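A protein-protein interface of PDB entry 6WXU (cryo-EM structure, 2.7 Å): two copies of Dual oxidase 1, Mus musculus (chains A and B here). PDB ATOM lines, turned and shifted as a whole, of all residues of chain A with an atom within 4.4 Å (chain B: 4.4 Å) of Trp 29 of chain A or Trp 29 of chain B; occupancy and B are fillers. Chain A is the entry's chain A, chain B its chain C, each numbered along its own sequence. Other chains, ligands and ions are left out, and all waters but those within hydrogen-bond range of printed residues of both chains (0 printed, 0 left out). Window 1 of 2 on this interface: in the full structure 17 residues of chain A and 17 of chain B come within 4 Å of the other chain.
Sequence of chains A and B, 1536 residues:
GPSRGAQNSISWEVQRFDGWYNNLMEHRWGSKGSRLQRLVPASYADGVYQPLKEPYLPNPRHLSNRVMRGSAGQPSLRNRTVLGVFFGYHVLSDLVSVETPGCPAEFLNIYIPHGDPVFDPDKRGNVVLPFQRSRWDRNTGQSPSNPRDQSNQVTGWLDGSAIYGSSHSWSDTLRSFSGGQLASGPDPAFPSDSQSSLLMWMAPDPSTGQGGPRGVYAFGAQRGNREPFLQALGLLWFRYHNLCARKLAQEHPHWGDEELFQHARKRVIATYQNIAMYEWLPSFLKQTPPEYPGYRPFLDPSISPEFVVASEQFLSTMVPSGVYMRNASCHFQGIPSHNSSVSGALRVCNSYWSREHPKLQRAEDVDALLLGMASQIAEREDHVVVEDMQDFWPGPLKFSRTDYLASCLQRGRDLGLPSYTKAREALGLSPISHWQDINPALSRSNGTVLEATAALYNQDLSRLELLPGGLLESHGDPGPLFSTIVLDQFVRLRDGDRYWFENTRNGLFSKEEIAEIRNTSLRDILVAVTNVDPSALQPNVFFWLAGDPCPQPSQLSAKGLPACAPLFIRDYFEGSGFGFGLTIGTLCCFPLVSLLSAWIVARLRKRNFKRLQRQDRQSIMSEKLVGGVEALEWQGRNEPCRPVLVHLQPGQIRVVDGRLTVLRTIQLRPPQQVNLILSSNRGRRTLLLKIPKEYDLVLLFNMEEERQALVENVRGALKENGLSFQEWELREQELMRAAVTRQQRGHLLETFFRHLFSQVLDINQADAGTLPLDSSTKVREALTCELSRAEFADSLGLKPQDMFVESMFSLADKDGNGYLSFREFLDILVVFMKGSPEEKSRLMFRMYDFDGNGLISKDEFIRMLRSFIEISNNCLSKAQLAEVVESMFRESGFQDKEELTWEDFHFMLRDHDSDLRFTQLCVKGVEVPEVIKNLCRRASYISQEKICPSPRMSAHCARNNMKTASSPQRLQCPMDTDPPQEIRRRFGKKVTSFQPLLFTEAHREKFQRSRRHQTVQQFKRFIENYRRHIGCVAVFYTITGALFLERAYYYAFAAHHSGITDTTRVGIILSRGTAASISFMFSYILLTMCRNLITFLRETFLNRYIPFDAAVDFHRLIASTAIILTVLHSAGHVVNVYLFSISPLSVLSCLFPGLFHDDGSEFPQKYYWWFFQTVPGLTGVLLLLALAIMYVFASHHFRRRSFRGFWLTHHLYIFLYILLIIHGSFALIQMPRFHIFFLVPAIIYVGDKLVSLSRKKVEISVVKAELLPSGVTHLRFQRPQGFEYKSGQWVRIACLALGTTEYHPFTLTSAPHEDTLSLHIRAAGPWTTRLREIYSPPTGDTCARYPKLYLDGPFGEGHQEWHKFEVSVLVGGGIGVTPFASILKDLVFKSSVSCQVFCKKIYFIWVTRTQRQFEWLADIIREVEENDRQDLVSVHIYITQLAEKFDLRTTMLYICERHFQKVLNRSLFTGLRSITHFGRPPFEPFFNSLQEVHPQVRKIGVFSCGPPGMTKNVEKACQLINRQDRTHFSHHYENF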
ATOM      1  N   GLY A  19      19.895  -3.579   5.764  1.00  0.00           N
ATOM      2  CA  GLY A  19      20.730  -2.433   6.040  1.00  0.00           C
ATOM      3  C   GLY A  19      21.662  -2.566   7.222  1.00  0.00           C
ATOM      4  O   GLY A  19      22.363  -1.601   7.540  1.00  0.00           O
ATOM      5  N   ASN A  23      27.923  -0.066   8.149  1.00  0.00           N
ATOM      6  CA  ASN A  23      28.974   0.734   8.753  1.00  0.00           C
ATOM      7  C   ASN A  23      29.782  -0.135   9.704  1.00  0.00           C
ATOM      8  O   ASN A  23      29.223  -0.971  10.417  1.00  0.00           O
ATOM      9  CB  ASN A  23      28.386   1.923   9.506  1.00  0.00           C
ATOM     10  CG  ASN A  23      29.295   3.118   9.496  1.00  0.00           C
ATOM     11  OD1 ASN A  23      29.751   3.546   8.445  1.00  0.00           O
ATOM     12  ND2 ASN A  23      29.576   3.659  10.666  1.00  0.00           N
ATOM     13  N   GLU A  26      29.105   1.802  13.605  1.00  0.00           N
ATOM     14  CA  GLU A  26      27.702   1.818  14.006  1.00  0.00           C
ATOM     15  C   GLU A  26      26.951   0.831  13.123  1.00  0.00           C
ATOM     16  O   GLU A  26      26.575   1.156  11.996  1.00  0.00           O
ATOM     17  CB  GLU A  26      27.132   3.225  13.890  1.00  0.00           C
ATOM     18  CG  GLU A  26      27.923   4.274  14.649  1.00  0.00           C
ATOM     19  CD  GLU A  26      27.584   4.307  16.120  1.00  0.00           C
ATOM     20  OE1 GLU A  26      26.579   3.684  16.512  1.00  0.00           O
ATOM     21  OE2 GLU A  26      28.318   4.959  16.887  1.00  0.00           O
ATOM     22  N   HIS A  27      26.726  -0.377  13.640  1.00  0.00           N
ATOM     23  CA  HIS A  27      26.110  -1.424  12.834  1.00  0.00           C
ATOM     24  C   HIS A  27      24.658  -1.119  12.515  1.00  0.00           C
ATOM     25  O   HIS A  27      24.148  -1.560  11.482  1.00  0.00           O
ATOM     26  CB  HIS A  27      26.195  -2.765  13.554  1.00  0.00           C
ATOM     27  CG  HIS A  27      27.590  -3.277  13.719  1.00  0.00           C
ATOM     28  ND1 HIS A  27      28.578  -3.054  12.788  1.00  0.00           N
ATOM     29  CD2 HIS A  27      28.159  -4.002  14.708  1.00  0.00           C
ATOM     30  CE1 HIS A  27      29.698  -3.620  13.197  1.00  0.00           C
ATOM     31  NE2 HIS A  27      29.472  -4.200  14.360  1.00  0.00           N
ATOM     32  N   ARG A  28      23.980  -0.379  13.380  1.00  0.00           N
ATOM     33  CA  ARG A  28      22.546  -0.176  13.266  1.00  0.00           C
ATOM     34  C   ARG A  28      22.169   1.005  12.384  1.00  0.00           C
ATOM     35  O   ARG A  28      20.979   1.214  12.141  1.00  0.00           O
ATOM     36  CB  ARG A  28      21.952   0.012  14.660  1.00  0.00           C
ATOM     37  CG  ARG A  28      20.541  -0.480  14.806  1.00  0.00           C
ATOM     38  CD  ARG A  28      20.116  -0.446  16.254  1.00  0.00           C
ATOM     39  NE  ARG A  28      21.051  -1.176  17.101  1.00  0.00           N
ATOM     40  CZ  ARG A  28      20.848  -1.427  18.388  1.00  0.00           C
ATOM     41  NH1 ARG A  28      21.751  -2.101  19.085  1.00  0.00           N
ATOM     42  NH2 ARG A  28      19.739  -1.008  18.977  1.00  0.00           N
ATOM     43  N   TRP A  29      23.137   1.779  11.902  1.00  0.00           N
ATOM     44  CA  TRP A  29      22.826   2.915  11.047  1.00  0.00           C
ATOM     45  C   TRP A  29      22.180   2.450   9.753  1.00  0.00           C
ATOM     46  O   TRP A  29      22.679   1.540   9.089  1.00  0.00           O
ATOM     47  CB  TRP A  29      24.092   3.707  10.731  1.00  0.00           C
ATOM     48  CG  TRP A  29      24.454   4.711  11.761  1.00  0.00           C
ATOM     49  CD1 TRP A  29      23.744   5.034  12.872  1.00  0.00           C
ATOM     50  CD2 TRP A  29      25.623   5.533  11.776  1.00  0.00           C
ATOM     51  NE1 TRP A  29      24.396   6.006  13.583  1.00  0.00           N
ATOM     52  CE2 TRP A  29      25.555   6.328  12.930  1.00  0.00           C
ATOM     53  CE3 TRP A  29      26.720   5.670  10.928  1.00  0.00           C
ATOM     54  CZ2 TRP A  29      26.542   7.247  13.257  1.00  0.00           C
ATOM     55  CZ3 TRP A  29      27.699   6.582  11.255  1.00  0.00           C
ATOM     56  CH2 TRP A  29      27.604   7.358  12.407  1.00  0.00           C
ATOM     57  N   GLY A  30      21.075   3.090   9.387  1.00  0.00           N
ATOM     58  CA  GLY A  30      20.394   2.783   8.153  1.00  0.00           C
ATOM     59  C   GLY A  30      19.534   1.544   8.174  1.00  0.00           C
ATOM     60  O   GLY A  30      18.784   1.320   7.221  1.00  0.00           O
ATOM     61  N   SER A  31      19.610   0.729   9.220  1.00  0.00           N
ATOM     62  CA  SER A  31      18.831  -0.494   9.271  1.00  0.00           C
ATOM     63  C   SER A  31      17.343  -0.174   9.331  1.00  0.00           C
ATOM     64  O   SER A  31      16.930   0.966   9.556  1.00  0.00           O
ATOM     65  CB  SER A  31      19.244  -1.335  10.472  1.00  0.00           C
ATOM     66  OG  SER A  31      19.058  -0.621  11.676  1.00  0.00           O
ATOM     67  N   TRP A 157      19.139   3.580   3.670  1.00  0.00           N
ATOM     68  CA  TRP A 157      20.080   3.667   2.566  1.00  0.00           C
ATOM     69  C   TRP A 157      19.337   3.737   1.242  1.00  0.00           C
ATOM     70  O   TRP A 157      18.204   3.268   1.117  1.00  0.00           O
ATOM     71  CB  TRP A 157      21.014   2.461   2.548  1.00  0.00           C
ATOM     72  CG  TRP A 157      21.702   2.200   3.823  1.00  0.00           C
ATOM     73  CD1 TRP A 157      21.460   1.182   4.684  1.00  0.00           C
ATOM     74  CD2 TRP A 157      22.762   2.967   4.393  1.00  0.00           C
ATOM     75  NE1 TRP A 157      22.300   1.264   5.760  1.00  0.00           N
ATOM     76  CE2 TRP A 157      23.112   2.355   5.603  1.00  0.00           C
ATOM     77  CE3 TRP A 157      23.449   4.116   3.997  1.00  0.00           C
ATOM     78  CZ2 TRP A 157      24.114   2.848   6.421  1.00  0.00           C
ATOM     79  CZ3 TRP A 157      24.438   4.601   4.807  1.00  0.00           C
ATOM     80  CH2 TRP A 157      24.766   3.968   6.006  1.00  0.00           C
ATOM     81  N   PRO A 297      33.546   7.171   6.591  1.00  0.00           N
ATOM     82  CA  PRO A 297      32.971   6.227   7.557  1.00  0.00           C
ATOM     83  C   PRO A 297      32.346   6.883   8.771  1.00  0.00           C
ATOM     84  O   PRO A 297      31.674   6.188   9.540  1.00  0.00           O
ATOM     85  CB  PRO A 297      34.174   5.370   7.964  1.00  0.00           C
ATOM     86  CG  PRO A 297      35.166   5.554   6.885  1.00  0.00           C
ATOM     87  CD  PRO A 297      34.982   6.941   6.388  1.00  0.00           C
ATOM     88  N   PHE A 298      32.534   8.186   8.971  1.00  0.00           N
ATOM     89  CA  PHE A 298      32.075   8.855  10.175  1.00  0.00           C
ATOM     90  C   PHE A 298      30.879   9.764   9.956  1.00  0.00           C
ATOM     91  O   PHE A 298      30.302  10.240  10.936  1.00  0.00           O
ATOM     92  CB  PHE A 298      33.219   9.665  10.792  1.00  0.00           C
ATOM     93  CG  PHE A 298      34.461   8.865  11.005  1.00  0.00           C
ATOM     94  CD1 PHE A 298      34.561   7.995  12.070  1.00  0.00           C
ATOM     95  CD2 PHE A 298      35.523   8.968  10.131  1.00  0.00           C
ATOM     96  CE1 PHE A 298      35.697   7.250  12.263  1.00  0.00           C
ATOM     97  CE2 PHE A 298      36.663   8.222  10.321  1.00  0.00           C
ATOM     98  CZ  PHE A 298      36.748   7.362  11.387  1.00  0.00           C
ATOM     99  N   LEU A 299      30.491  10.019   8.713  1.00  0.00           N
ATOM    100  CA  LEU A 299      29.279  10.780   8.458  1.00  0.00           C
ATOM    101  C   LEU A 299      28.062   9.989   8.909  1.00  0.00           C
ATOM    102  O   LEU A 299      27.942   8.797   8.621  1.00  0.00           O
ATOM    103  CB  LEU A 299      29.160  11.117   6.978  1.00  0.00           C
ATOM    104  CG  LEU A 299      29.421  12.565   6.598  1.00  0.00           C
ATOM    105  CD1 LEU A 299      28.975  12.793   5.178  1.00  0.00           C
ATOM    106  CD2 LEU A 299      28.694  13.490   7.543  1.00  0.00           C
ATOM    107  N   ASP A 300      27.159  10.654   9.618  1.00  0.00           N
ATOM    108  CA  ASP A 300      25.918  10.033  10.055  1.00  0.00           C
ATOM    109  C   ASP A 300      24.877  10.173   8.955  1.00  0.00           C
ATOM    110  O   ASP A 300      24.501  11.303   8.618  1.00  0.00           O
ATOM    111  CB  ASP A 300      25.426  10.681  11.335  1.00  0.00           C
ATOM    112  CG  ASP A 300      24.296   9.921  11.982  1.00  0.00           C
ATOM    113  OD1 ASP A 300      23.802   8.948  11.390  1.00  0.00           O
ATOM    114  OD2 ASP A 300      23.898  10.301  13.098  1.00  0.00           O
ATOM    115  N   PRO A 301      24.395   9.080   8.370  1.00  0.00           N
ATOM    116  CA  PRO A 301      23.468   9.169   7.235  1.00  0.00           C
ATOM    117  C   PRO A 301      21.993   9.116   7.600  1.00  0.00           C
ATOM    118  O   PRO A 301      21.170   8.958   6.696  1.00  0.00           O
ATOM    119  CB  PRO A 301      23.854   7.926   6.435  1.00  0.00           C
ATOM    120  CG  PRO A 301      24.120   6.936   7.505  1.00  0.00           C
ATOM    121  CD  PRO A 301      24.770   7.684   8.636  1.00  0.00           C
ATOM    122  N   SER A 302      21.643   9.231   8.877  1.00  0.00           N
ATOM    123  CA  SER A 302      20.280   8.990   9.316  1.00  0.00           C
ATOM    124  C   SER A 302      19.309   9.963   8.662  1.00  0.00           C
ATOM    125  O   SER A 302      19.682  11.031   8.176  1.00  0.00           O
ATOM    126  CB  SER A 302      20.183   9.102  10.832  1.00  0.00           C
ATOM    127  OG  SER A 302      21.019   8.148  11.456  1.00  0.00           O
ATOM    128  N   GLY B  19      30.322  13.667  29.897  1.00  0.00           N
ATOM    129  CA  GLY B  19      30.255  13.689  28.453  1.00  0.00           C
ATOM    130  C   GLY B  19      28.943  13.245  27.849  1.00  0.00           C
ATOM    131  O   GLY B  19      28.841  13.191  26.619  1.00  0.00           O
ATOM    132  N   ASN B  23      25.757  15.426  22.245  1.00  0.00           N
ATOM    133  CA  ASN B  23      25.185  15.356  20.912  1.00  0.00           C
ATOM    134  C   ASN B  23      23.681  15.164  21.020  1.00  0.00           C
ATOM    135  O   ASN B  23      23.204  14.424  21.883  1.00  0.00           O
ATOM    136  CB  ASN B  23      25.801  14.209  20.118  1.00  0.00           C
ATOM    137  CG  ASN B  23      25.867  14.497  18.646  1.00  0.00           C
ATOM    138  OD1 ASN B  23      26.371  15.532  18.235  1.00  0.00           O
ATOM    139  ND2 ASN B  23      25.346  13.591  17.840  1.00  0.00           N
ATOM    140  N   GLU B  26      23.058  11.248  19.097  1.00  0.00           N
ATOM    141  CA  GLU B  26      23.754  10.156  19.770  1.00  0.00           C
ATOM    142  C   GLU B  26      24.182  10.651  21.145  1.00  0.00           C
ATOM    143  O   GLU B  26      25.209  11.316  21.283  1.00  0.00           O
ATOM    144  CB  GLU B  26      24.946   9.695  18.942  1.00  0.00           C
ATOM    145  CG  GLU B  26      24.593   9.313  17.517  1.00  0.00           C
ATOM    146  CD  GLU B  26      24.035   7.914  17.409  1.00  0.00           C
ATOM    147  OE1 GLU B  26      24.134   7.159  18.395  1.00  0.00           O
ATOM    148  OE2 GLU B  26      23.500   7.564  16.340  1.00  0.00           O
ATOM    149  N   HIS B  27      23.395  10.318  22.168  1.00  0.00           N
ATOM    150  CA  HIS B  27      23.661  10.832  23.506  1.00  0.00           C
ATOM    151  C   HIS B  27      24.936  10.255  24.096  1.00  0.00           C
ATOM    152  O   HIS B  27      25.583  10.906  24.918  1.00  0.00           O
ATOM    153  CB  HIS B  27      22.493  10.523  24.434  1.00  0.00           C
ATOM    154  CG  HIS B  27      21.228  11.232  24.072  1.00  0.00           C
ATOM    155  ND1 HIS B  27      21.213  12.493  23.522  1.00  0.00           N
ATOM    156  CD2 HIS B  27      19.934  10.854  24.184  1.00  0.00           C
ATOM    157  CE1 HIS B  27      19.964  12.862  23.309  1.00  0.00           C
ATOM    158  NE2 HIS B  27      19.169  11.885  23.700  1.00  0.00           N
ATOM    159  N   ARG B  28      25.306   9.047  23.699  1.00  0.00           N
ATOM    160  CA  ARG B  28      26.402   8.329  24.327  1.00  0.00           C
ATOM    161  C   ARG B  28      27.760   8.642  23.717  1.00  0.00           C
ATOM    162  O   ARG B  28      28.772   8.161  24.231  1.00  0.00           O
ATOM    163  CB  ARG B  28      26.133   6.829  24.245  1.00  0.00           C
ATOM    164  CG  ARG B  28      26.698   6.031  25.385  1.00  0.00           C
ATOM    165  CD  ARG B  28      26.208   4.606  25.328  1.00  0.00           C
ATOM    166  NE  ARG B  28      24.754   4.544  25.273  1.00  0.00           N
ATOM    167  CZ  ARG B  28      24.053   3.419  25.359  1.00  0.00           C
ATOM    168  NH1 ARG B  28      22.730   3.453  25.302  1.00  0.00           N
ATOM    169  NH2 ARG B  28      24.677   2.262  25.507  1.00  0.00           N
ATOM    170  N   TRP B  29      27.813   9.425  22.643  1.00  0.00           N
ATOM    171  CA  TRP B  29      29.091   9.759  22.030  1.00  0.00           C
ATOM    172  C   TRP B  29      29.955  10.557  22.992  1.00  0.00           C
ATOM    173  O   TRP B  29      29.499  11.533  23.590  1.00  0.00           O
ATOM    174  CB  TRP B  29      28.873  10.564  20.751  1.00  0.00           C
ATOM    175  CG  TRP B  29      28.626   9.736  19.546  1.00  0.00           C
ATOM    176  CD1 TRP B  29      28.659   8.381  19.466  1.00  0.00           C
ATOM    177  CD2 TRP B  29      28.308  10.209  18.236  1.00  0.00           C
ATOM    178  NE1 TRP B  29      28.379   7.977  18.187  1.00  0.00           N
ATOM    179  CE2 TRP B  29      28.159   9.084  17.413  1.00  0.00           C
ATOM    180  CE3 TRP B  29      28.132  11.477  17.682  1.00  0.00           C
ATOM    181  CZ2 TRP B  29      27.843   9.187  16.065  1.00  0.00           C
ATOM    182  CZ3 TRP B  29      27.819  11.575  16.344  1.00  0.00           C
ATOM    183  CH2 TRP B  29      27.677  10.439  15.552  1.00  0.00           C
ATOM    184  N   GLY B  30      31.211  10.147  23.128  1.00  0.00           N
ATOM    185  CA  GLY B  30      32.151  10.848  23.968  1.00  0.00           C
ATOM    186  C   GLY B  30      32.023  10.585  25.447  1.00  0.00           C
ATOM    187  O   GLY B  30      32.902  11.002  26.207  1.00  0.00           O
ATOM    188  N   SER B  31      30.969   9.910  25.890  1.00  0.00           N
ATOM    189  CA  SER B  31      30.783   9.662  27.308  1.00  0.00           C
ATOM    190  C   SER B  31      31.883   8.751  27.838  1.00  0.00           C
ATOM    191  O   SER B  31      32.644   8.142  27.083  1.00  0.00           O
ATOM    192  CB  SER B  31      29.414   9.046  27.563  1.00  0.00           C
ATOM    193  OG  SER B  31      29.269   7.830  26.861  1.00  0.00           O
ATOM    194  N   TRP B 157      35.813  13.715  24.791  1.00  0.00           N
ATOM    195  CA  TRP B 157      35.849  15.116  24.408  1.00  0.00           C
ATOM    196  C   TRP B 157      37.081  15.792  24.988  1.00  0.00           C
ATOM    197  O   TRP B 157      37.626  15.364  26.008  1.00  0.00           O
ATOM    198  CB  TRP B 157      34.605  15.850  24.898  1.00  0.00           C
ATOM    199  CG  TRP B 157      33.331  15.219  24.514  1.00  0.00           C
ATOM    200  CD1 TRP B 157      32.471  14.560  25.328  1.00  0.00           C
ATOM    201  CD2 TRP B 157      32.754  15.188  23.209  1.00  0.00           C
ATOM    202  NE1 TRP B 157      31.393  14.115  24.615  1.00  0.00           N
ATOM    203  CE2 TRP B 157      31.543  14.491  23.307  1.00  0.00           C
ATOM    204  CE3 TRP B 157      33.146  15.682  21.964  1.00  0.00           C
ATOM    205  CZ2 TRP B 157      30.723  14.273  22.215  1.00  0.00           C
ATOM    206  CZ3 TRP B 157      32.333  15.466  20.886  1.00  0.00           C
ATOM    207  CH2 TRP B 157      31.132  14.769  21.015  1.00  0.00           C
ATOM    208  N   PRO B 297      26.885  18.469  13.534  1.00  0.00           N
ATOM    209  CA  PRO B 297      26.223  17.531  14.449  1.00  0.00           C
ATOM    210  C   PRO B 297      26.325  16.078  14.031  1.00  0.00           C
ATOM    211  O   PRO B 297      25.967  15.205  14.828  1.00  0.00           O
ATOM    212  CB  PRO B 297      24.765  17.998  14.432  1.00  0.00           C
ATOM    213  CG  PRO B 297      24.807  19.389  13.936  1.00  0.00           C
ATOM    214  CD  PRO B 297      25.944  19.454  12.984  1.00  0.00           C
ATOM    215  N   PHE B 298      26.801  15.786  12.822  1.00  0.00           N
ATOM    216  CA  PHE B 298      26.809  14.429  12.304  1.00  0.00           C
ATOM    217  C   PHE B 298      28.190  13.802  12.242  1.00  0.00           C
ATOM    218  O   PHE B 298      28.290  12.600  11.987  1.00  0.00           O
ATOM    219  CB  PHE B 298      26.176  14.396  10.910  1.00  0.00           C
ATOM    220  CG  PHE B 298      24.827  15.035  10.859  1.00  0.00           C
ATOM    221  CD1 PHE B 298      23.718  14.366  11.331  1.00  0.00           C
ATOM    222  CD2 PHE B 298      24.670  16.310  10.356  1.00  0.00           C
ATOM    223  CE1 PHE B 298      22.477  14.953  11.295  1.00  0.00           C
ATOM    224  CE2 PHE B 298      23.429  16.901  10.320  1.00  0.00           C
ATOM    225  CZ  PHE B 298      22.334  16.222  10.792  1.00  0.00           C
ATOM    226  N   LEU B 299      29.249  14.569  12.463  1.00  0.00           N
ATOM    227  CA  LEU B 299      30.580  13.989  12.537  1.00  0.00           C
ATOM    228  C   LEU B 299      30.694  13.099  13.766  1.00  0.00           C
ATOM    229  O   LEU B 299      30.283  13.483  14.862  1.00  0.00           O
ATOM    230  CB  LEU B 299      31.638  15.082  12.589  1.00  0.00           C
ATOM    231  CG  LEU B 299      32.458  15.280  11.325  1.00  0.00           C
ATOM    232  CD1 LEU B 299      33.637  16.167  11.631  1.00  0.00           C
ATOM    233  CD2 LEU B 299      32.917  13.947  10.788  1.00  0.00           C
ATOM    234  N   ASP B 300      31.253  11.910  13.579  1.00  0.00           N
ATOM    235  CA  ASP B 300      31.481  10.990  14.682  1.00  0.00           C
ATOM    236  C   ASP B 300      32.822  11.307  15.325  1.00  0.00           C
ATOM    237  O   ASP B 300      33.858  11.181  14.660  1.00  0.00           O
ATOM    238  CB  ASP B 300      31.457   9.558  14.186  1.00  0.00           C
ATOM    239  CG  ASP B 300      31.426   8.548  15.306  1.00  0.00           C
ATOM    240  OD1 ASP B 300      31.538   8.939  16.480  1.00  0.00           O
ATOM    241  OD2 ASP B 300      31.286   7.348  15.010  1.00  0.00           O
ATOM    242  N   PRO B 301      32.858  11.721  16.590  1.00  0.00           N
ATOM    243  CA  PRO B 301      34.117  12.137  17.219  1.00  0.00           C
ATOM    244  C   PRO B 301      34.842  11.049  17.995  1.00  0.00           C
ATOM    245  O   PRO B 301      35.776  11.375  18.731  1.00  0.00           O
ATOM    246  CB  PRO B 301      33.628  13.223  18.176  1.00  0.00           C
ATOM    247  CG  PRO B 301      32.343  12.661  18.656  1.00  0.00           C
ATOM    248  CD  PRO B 301      31.718  11.951  17.487  1.00  0.00           C
ATOM    249  N   SER B 302      34.441   9.788  17.861  1.00  0.00           N
ATOM    250  CA  SER B 302      34.953   8.733  18.717  1.00  0.00           C
ATOM    251  C   SER B 302      36.458   8.574  18.559  1.00  0.00           C
ATOM    252  O   SER B 302      37.057   8.987  17.566  1.00  0.00           O
ATOM    253  CB  SER B 302      34.256   7.415  18.407  1.00  0.00           C
ATOM    254  OG  SER B 302      32.865   7.521  18.629  1.00  0.00           O
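The backbone NH (N) of Asp 300 of chain B sits at hydrogen-bond distance from the backbone carbonyl oxygen (O) of Phe 298 of chain A, at 3.3 Å. The indole nitrogen (NE1) of Trp 29 of chain A sits at hydrogen-bond distance from the side-chain carboxylate (OE2) of Glu 26 of chain B, 3.3 Å away. O of Phe 298 of chain B is in hydrogen-bond range of N of Asp 300 of chain A, at 3.3 Å. OE2 of Glu 26 of chain A sits at hydrogen-bond distance from NE1 of Trp 29 of chain B (3.3 Å). The backbone carbonyl oxygen of Phe 298 of chain B sits close to the backbone carbonyl oxygen of Phe 298 of chain A (3.3 Å).
The indole nitrogen (NE1) of Trp 157 of chain A lies close to the backbone carbonyl oxygen (O) of Trp 29 of chain A. The side-chain carboxylate (OD1) of Asp 300 of chain A is in hydrogen-bond range of the side-chain hydroxyl (OG) of Ser 302 of chain A, at 2.9 Å. The backbone carbonyl oxygen of Trp 29 of chain B lies close to the indole nitrogen of Trp 157 of chain B (3.4 Å). The side-chain carboxylate (OD1) of Asp 300 of chain B lies within hydrogen-bond range of the side-chain hydroxyl (OG) of Ser 302 of chain B, at 2.9 Å.
Among the printed residues, merely in contact across the chains: Trp 29 of chain A with Trp 29 of chain B.
Printed residues of chain B within 4 Å of Glu 26 of chain A: Trp 29 (3.3 Å). Trp 29 of chain A touches two residues of chain B. Printed residues of chain B within 4 Å of Phe 298 of chain A: Phe 298 and Asp 300. Trp 29 of chain B touches just these residues of chain A: Glu 26 and Trp 29. Printed residues of chain A within 4 Å of Phe 298 of chain B: Phe 298 and Asp 300. Of the printed residues of chain A, Asp 300 of chain B touches Phe 298. The nearest printed residue of chain A that does not touch Trp 29 of chain B is Asp 300 of chain A (4.5 Å). The nearest printed residue of chain A that does not touch Glu 26 of chain B is Asp 300 of chain A (4.3 Å).
Printed residues of chain A that touch a printed residue of chain B: Glu 26, Trp 29, Phe 298 and Asp 300. Along chain A the printed residues that touch a printed residue of chain B span positions 26 to 300. Of the 15 printed residues of chain B, 4 touch a printed residue of chain A. Hydrophobic or aromatic side chains of chain B within 4 Å of the printed part of chain A: Trp 29 and Phe 298. Among the printed residues, 6 pairs touch across the chains.
Glu 26 of chain A touches Trp 29 of chain B, and with the chains exchanged Trp 29 of chain A touches Glu 26 of chain B. Trp 29 of chain B touches its own counterpart, Trp 29 of chain A. Phe 298 of chain B touches its own counterpart, Phe 298 of chain A. Phe 298 of chain A touches Asp 300 of chain B, and with the chains exchanged Asp 300 of chain A touches Phe 298 of chain B. 15 positions are printed for both chains. Of the 6 pairs that touch across the chains among the printed residues, 6 have their exchanged pair printed and touching as well.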
